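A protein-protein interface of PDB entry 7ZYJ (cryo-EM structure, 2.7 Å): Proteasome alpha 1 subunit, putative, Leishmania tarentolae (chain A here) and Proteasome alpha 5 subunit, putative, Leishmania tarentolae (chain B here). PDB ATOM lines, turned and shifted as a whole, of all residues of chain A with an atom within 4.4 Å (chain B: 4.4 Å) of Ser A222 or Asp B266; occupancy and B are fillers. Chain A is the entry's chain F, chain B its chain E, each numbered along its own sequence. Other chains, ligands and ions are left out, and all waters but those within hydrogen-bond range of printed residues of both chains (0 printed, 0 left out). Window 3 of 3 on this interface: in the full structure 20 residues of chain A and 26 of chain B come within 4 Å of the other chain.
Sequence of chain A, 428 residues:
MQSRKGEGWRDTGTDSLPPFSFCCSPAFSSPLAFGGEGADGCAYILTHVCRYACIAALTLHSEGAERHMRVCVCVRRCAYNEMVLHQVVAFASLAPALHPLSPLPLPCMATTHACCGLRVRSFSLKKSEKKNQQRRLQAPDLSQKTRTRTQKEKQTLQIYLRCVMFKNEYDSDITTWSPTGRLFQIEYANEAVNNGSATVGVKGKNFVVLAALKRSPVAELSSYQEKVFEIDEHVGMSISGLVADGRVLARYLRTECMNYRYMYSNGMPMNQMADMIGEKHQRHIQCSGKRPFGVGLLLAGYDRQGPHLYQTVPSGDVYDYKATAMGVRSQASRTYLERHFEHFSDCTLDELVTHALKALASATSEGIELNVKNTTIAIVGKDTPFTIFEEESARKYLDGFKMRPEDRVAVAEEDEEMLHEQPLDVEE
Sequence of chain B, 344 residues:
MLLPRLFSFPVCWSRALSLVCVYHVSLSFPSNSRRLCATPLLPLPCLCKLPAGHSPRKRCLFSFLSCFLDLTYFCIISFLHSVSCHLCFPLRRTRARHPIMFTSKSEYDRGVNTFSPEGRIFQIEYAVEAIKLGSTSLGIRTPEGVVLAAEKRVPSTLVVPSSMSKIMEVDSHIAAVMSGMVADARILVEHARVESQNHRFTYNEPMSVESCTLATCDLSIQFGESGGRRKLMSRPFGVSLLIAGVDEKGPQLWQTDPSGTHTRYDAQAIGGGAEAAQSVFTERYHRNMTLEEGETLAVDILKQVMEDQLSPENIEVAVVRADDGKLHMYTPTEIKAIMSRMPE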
ATOM      1  N   PRO A 217      16.212   2.397 -20.491  1.00  0.00           N
ATOM      2  CA  PRO A 217      16.419   1.222 -21.344  1.00  0.00           C
ATOM      3  C   PRO A 217      15.602   1.310 -22.622  1.00  0.00           C
ATOM      4  O   PRO A 217      14.540   1.935 -22.663  1.00  0.00           O
ATOM      5  CB  PRO A 217      15.949   0.053 -20.467  1.00  0.00           C
ATOM      6  CG  PRO A 217      15.874   0.603 -19.071  1.00  0.00           C
ATOM      7  CD  PRO A 217      15.562   2.051 -19.217  1.00  0.00           C
ATOM      8  N   GLU A 220      14.019  -3.229 -23.454  1.00  0.00           N
ATOM      9  CA  GLU A 220      14.531  -4.422 -22.790  1.00  0.00           C
ATOM     10  C   GLU A 220      15.968  -4.268 -22.306  1.00  0.00           C
ATOM     11  O   GLU A 220      16.437  -5.060 -21.483  1.00  0.00           O
ATOM     12  CB  GLU A 220      14.429  -5.633 -23.716  1.00  0.00           C
ATOM     13  CG  GLU A 220      14.296  -6.940 -22.962  1.00  0.00           C
ATOM     14  CD  GLU A 220      13.006  -7.038 -22.173  1.00  0.00           C
ATOM     15  OE1 GLU A 220      11.991  -6.461 -22.608  1.00  0.00           O
ATOM     16  OE2 GLU A 220      13.014  -7.680 -21.100  1.00  0.00           O
ATOM     17  N   LEU A 221      16.679  -3.266 -22.816  1.00  0.00           N
ATOM     18  CA  LEU A 221      18.128  -3.181 -22.681  1.00  0.00           C
ATOM     19  C   LEU A 221      18.491  -2.004 -21.791  1.00  0.00           C
ATOM     20  O   LEU A 221      18.495  -0.859 -22.248  1.00  0.00           O
ATOM     21  CB  LEU A 221      18.788  -3.033 -24.052  1.00  0.00           C
ATOM     22  CG  LEU A 221      18.412  -4.086 -25.098  1.00  0.00           C
ATOM     23  CD1 LEU A 221      17.301  -3.583 -26.013  1.00  0.00           C
ATOM     24  CD2 LEU A 221      19.623  -4.500 -25.916  1.00  0.00           C
ATOM     25  N   SER A 222      18.837  -2.291 -20.538  1.00  0.00           N
ATOM     26  CA  SER A 222      19.168  -1.265 -19.558  1.00  0.00           C
ATOM     27  C   SER A 222      20.677  -1.046 -19.549  1.00  0.00           C
ATOM     28  O   SER A 222      21.438  -1.931 -19.145  1.00  0.00           O
ATOM     29  CB  SER A 222      18.666  -1.661 -18.172  1.00  0.00           C
ATOM     30  OG  SER A 222      19.205  -2.911 -17.782  1.00  0.00           O
ATOM     31  N   SER A 223      21.101   0.135 -19.990  1.00  0.00           N
ATOM     32  CA  SER A 223      22.499   0.535 -19.938  1.00  0.00           C
ATOM     33  C   SER A 223      22.734   1.397 -18.706  1.00  0.00           C
ATOM     34  O   SER A 223      21.933   2.286 -18.402  1.00  0.00           O
ATOM     35  CB  SER A 223      22.892   1.299 -21.202  1.00  0.00           C
ATOM     36  OG  SER A 223      22.249   2.562 -21.259  1.00  0.00           O
ATOM     37  N   TYR A 224      23.832   1.137 -18.003  1.00  0.00           N
ATOM     38  CA  TYR A 224      24.178   1.867 -16.794  1.00  0.00           C
ATOM     39  C   TYR A 224      25.485   2.616 -16.996  1.00  0.00           C
ATOM     40  O   TYR A 224      26.459   2.062 -17.516  1.00  0.00           O
ATOM     41  CB  TYR A 224      24.298   0.929 -15.590  1.00  0.00           C
ATOM     42  CG  TYR A 224      24.946   1.574 -14.388  1.00  0.00           C
ATOM     43  CD1 TYR A 224      24.229   2.438 -13.571  1.00  0.00           C
ATOM     44  CD2 TYR A 224      26.274   1.323 -14.070  1.00  0.00           C
ATOM     45  CE1 TYR A 224      24.817   3.033 -12.472  1.00  0.00           C
ATOM     46  CE2 TYR A 224      26.870   1.914 -12.974  1.00  0.00           C
ATOM     47  CZ  TYR A 224      26.136   2.767 -12.178  1.00  0.00           C
ATOM     48  OH  TYR A 224      26.726   3.355 -11.086  1.00  0.00           O
ATOM     49  N   GLY B 139      27.586  -9.453 -27.515  1.00  0.00           N
ATOM     50  CA  GLY B 139      27.622  -9.753 -26.097  1.00  0.00           C
ATOM     51  C   GLY B 139      26.229  -9.873 -25.515  1.00  0.00           C
ATOM     52  O   GLY B 139      25.397  -8.983 -25.704  1.00  0.00           O
ATOM     53  N   ILE B 140      25.962 -10.967 -24.804  1.00  0.00           N
ATOM     54  CA  ILE B 140      24.648 -11.250 -24.239  1.00  0.00           C
ATOM     55  C   ILE B 140      24.817 -11.576 -22.764  1.00  0.00           C
ATOM     56  O   ILE B 140      25.635 -12.429 -22.407  1.00  0.00           O
ATOM     57  CB  ILE B 140      23.951 -12.420 -24.960  1.00  0.00           C
ATOM     58  CG1 ILE B 140      23.937 -12.198 -26.471  1.00  0.00           C
ATOM     59  CG2 ILE B 140      22.534 -12.597 -24.438  1.00  0.00           C
ATOM     60  CD1 ILE B 140      23.120 -11.016 -26.892  1.00  0.00           C
ATOM     61  N   ARG B 141      24.039 -10.915 -21.914  1.00  0.00           N
ATOM     62  CA  ARG B 141      24.037 -11.181 -20.482  1.00  0.00           C
ATOM     63  C   ARG B 141      22.740 -11.883 -20.106  1.00  0.00           C
ATOM     64  O   ARG B 141      21.653 -11.404 -20.444  1.00  0.00           O
ATOM     65  CB  ARG B 141      24.193  -9.887 -19.682  1.00  0.00           C
ATOM     66  CG  ARG B 141      24.427 -10.102 -18.196  1.00  0.00           C
ATOM     67  CD  ARG B 141      23.674  -9.079 -17.365  1.00  0.00           C
ATOM     68  NE  ARG B 141      22.238  -9.332 -17.359  1.00  0.00           N
ATOM     69  CZ  ARG B 141      21.633 -10.198 -16.557  1.00  0.00           C
ATOM     70  NH1 ARG B 141      22.312 -10.916 -15.679  1.00  0.00           N
ATOM     71  NH2 ARG B 141      20.313 -10.344 -16.638  1.00  0.00           N
ATOM     72  N   LEU B 253      28.404  -7.565 -18.208  1.00  0.00           N
ATOM     73  CA  LEU B 253      28.922  -7.212 -19.522  1.00  0.00           C
ATOM     74  C   LEU B 253      29.103  -5.705 -19.590  1.00  0.00           C
ATOM     75  O   LEU B 253      28.184  -4.950 -19.254  1.00  0.00           O
ATOM     76  CB  LEU B 253      27.981  -7.687 -20.633  1.00  0.00           C
ATOM     77  CG  LEU B 253      28.248  -7.132 -22.032  1.00  0.00           C
ATOM     78  CD1 LEU B 253      29.561  -7.669 -22.569  1.00  0.00           C
ATOM     79  CD2 LEU B 253      27.104  -7.466 -22.971  1.00  0.00           C
ATOM     80  N   ARG B 264      27.935  -0.286 -18.619  1.00  0.00           N
ATOM     81  CA  ARG B 264      27.389  -1.616 -18.387  1.00  0.00           C
ATOM     82  C   ARG B 264      26.190  -1.840 -19.297  1.00  0.00           C
ATOM     83  O   ARG B 264      25.325  -0.967 -19.423  1.00  0.00           O
ATOM     84  CB  ARG B 264      26.987  -1.783 -16.923  1.00  0.00           C
ATOM     85  CG  ARG B 264      26.505  -3.177 -16.567  1.00  0.00           C
ATOM     86  CD  ARG B 264      26.153  -3.275 -15.092  1.00  0.00           C
ATOM     87  NE  ARG B 264      24.998  -2.454 -14.749  1.00  0.00           N
ATOM     88  CZ  ARG B 264      24.667  -2.109 -13.513  1.00  0.00           C
ATOM     89  NH1 ARG B 264      25.391  -2.486 -12.472  1.00  0.00           N
ATOM     90  NH2 ARG B 264      23.583  -1.364 -13.315  1.00  0.00           N
ATOM     91  N   TYR B 265      26.135  -3.006 -19.931  1.00  0.00           N
ATOM     92  CA  TYR B 265      25.099  -3.318 -20.902  1.00  0.00           C
ATOM     93  C   TYR B 265      24.485  -4.679 -20.605  1.00  0.00           C
ATOM     94  O   TYR B 265      25.082  -5.531 -19.941  1.00  0.00           O
ATOM     95  CB  TYR B 265      25.659  -3.304 -22.330  1.00  0.00           C
ATOM     96  CG  TYR B 265      25.698  -1.938 -22.970  1.00  0.00           C
ATOM     97  CD1 TYR B 265      24.535  -1.326 -23.419  1.00  0.00           C
ATOM     98  CD2 TYR B 265      26.898  -1.261 -23.133  1.00  0.00           C
ATOM     99  CE1 TYR B 265      24.568  -0.077 -24.007  1.00  0.00           C
ATOM    100  CE2 TYR B 265      26.941  -0.015 -23.720  1.00  0.00           C
ATOM    101  CZ  TYR B 265      25.774   0.574 -24.153  1.00  0.00           C
ATOM    102  OH  TYR B 265      25.813   1.817 -24.740  1.00  0.00           O
ATOM    103  N   ASP B 266      23.272  -4.871 -21.111  1.00  0.00           N
ATOM    104  CA  ASP B 266      22.602  -6.165 -21.100  1.00  0.00           C
ATOM    105  C   ASP B 266      22.805  -6.940 -22.390  1.00  0.00           C
ATOM    106  O   ASP B 266      22.951  -8.163 -22.356  1.00  0.00           O
ATOM    107  CB  ASP B 266      21.100  -5.981 -20.852  1.00  0.00           C
ATOM    108  CG  ASP B 266      20.779  -5.701 -19.398  1.00  0.00           C
ATOM    109  OD1 ASP B 266      21.196  -6.496 -18.531  1.00  0.00           O
ATOM    110  OD2 ASP B 266      20.108  -4.685 -19.123  1.00  0.00           O
ATOM    111  N   ALA B 267      22.817  -6.248 -23.528  1.00  0.00           N
ATOM    112  CA  ALA B 267      23.123  -6.872 -24.813  1.00  0.00           C
ATOM    113  C   ALA B 267      23.626  -5.776 -25.741  1.00  0.00           C
ATOM    114  O   ALA B 267      22.832  -4.955 -26.211  1.00  0.00           O
ATOM    115  CB  ALA B 267      21.898  -7.571 -25.388  1.00  0.00           C
ATOM    116  N   GLN B 268      24.928  -5.761 -26.002  1.00  0.00           N
ATOM    117  CA  GLN B 268      25.549  -4.732 -26.820  1.00  0.00           C
ATOM    118  C   GLN B 268      26.299  -5.365 -27.983  1.00  0.00           C
ATOM    119  O   GLN B 268      26.857  -6.460 -27.864  1.00  0.00           O
ATOM    120  CB  GLN B 268      26.506  -3.863 -25.987  1.00  0.00           C
ATOM    121  CG  GLN B 268      27.199  -2.742 -26.758  1.00  0.00           C
ATOM    122  CD  GLN B 268      26.233  -1.857 -27.523  1.00  0.00           C
ATOM    123  OE1 GLN B 268      25.818  -2.181 -28.635  1.00  0.00           O
ATOM    124  NE2 GLN B 268      25.876  -0.725 -26.932  1.00  0.00           N
ATOM    125  N   TYR B 285      14.630 -10.588 -27.141  1.00  0.00           N
ATOM    126  CA  TYR B 285      15.526 -10.583 -25.988  1.00  0.00           C
ATOM    127  C   TYR B 285      14.720 -10.238 -24.746  1.00  0.00           C
ATOM    128  O   TYR B 285      13.817  -9.399 -24.809  1.00  0.00           O
ATOM    129  CB  TYR B 285      16.673  -9.585 -26.183  1.00  0.00           C
ATOM    130  CG  TYR B 285      17.526  -9.376 -24.950  1.00  0.00           C
ATOM    131  CD1 TYR B 285      18.572 -10.237 -24.660  1.00  0.00           C
ATOM    132  CD2 TYR B 285      17.301  -8.309 -24.090  1.00  0.00           C
ATOM    133  CE1 TYR B 285      19.355 -10.062 -23.543  1.00  0.00           C
ATOM    134  CE2 TYR B 285      18.083  -8.122 -22.967  1.00  0.00           C
ATOM    135  CZ  TYR B 285      19.109  -9.002 -22.700  1.00  0.00           C
ATOM    136  OH  TYR B 285      19.896  -8.829 -21.588  1.00  0.00           O
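Hydrophobic or aromatic side chains of chain B within 4 Å of the printed part of chain A: Tyr B265, Ala B267 and Tyr B285.
Of the printed residues of chain B, Leu A221 touches Ala B267.
Of the printed residues of chain B, Ser A222 touches Asp B266.
Of the printed residues of chain B, Ser A223 touches Arg B264 and Tyr B265.
Arg B141 touches none of the printed residues of chain A.
Printed residues of chain A within 4 Å of Arg B264: Ser A223 and Tyr A224.
Of chain A, only Ser A222 comes within 4 Å of Asp B266.
Of the printed residues of chain A, Tyr B285 touches Glu A220.
The nearest printed residue of chain B that does not touch Ser A222 is Arg B264 (4.01 Å).
The guanidinium group of Arg B141 is in salt-bridge range of the side-chain carboxylate of Asp B266.
OH of Tyr B285 sits at hydrogen-bond distance from O of Arg B141 (3.3 Å).
The backbone NH (N) of Tyr B265 is in hydrogen-bond range of the backbone carbonyl oxygen (O) of Leu B253 (2.9 Å).
OH of Tyr B265 lies close to NE2 of Gln B268 (3.4 Å).
OH of Tyr B285 lies close to O of Asp B266 (3.2 Å).
The backbone carbonyl oxygen (O) of Arg B264 is in hydrogen-bond range of the backbone NH (N) of Tyr A224, at 2.9 Å.
The side-chain hydroxyl (OG) of Ser A222 sits at hydrogen-bond distance from the side-chain carboxylate (OD2) of Asp B266.
Tyr B285 touches Glu A220 (O to CG, 3.1 Å).
Leu A221 touches Ala B267 (CD2 to O, 3.3 Å).
Ser A223 touches Arg B264 (CA to O, 3.2 Å).
CB of Ser A223 touches CE1 of Tyr B265, at 3.5 Å.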
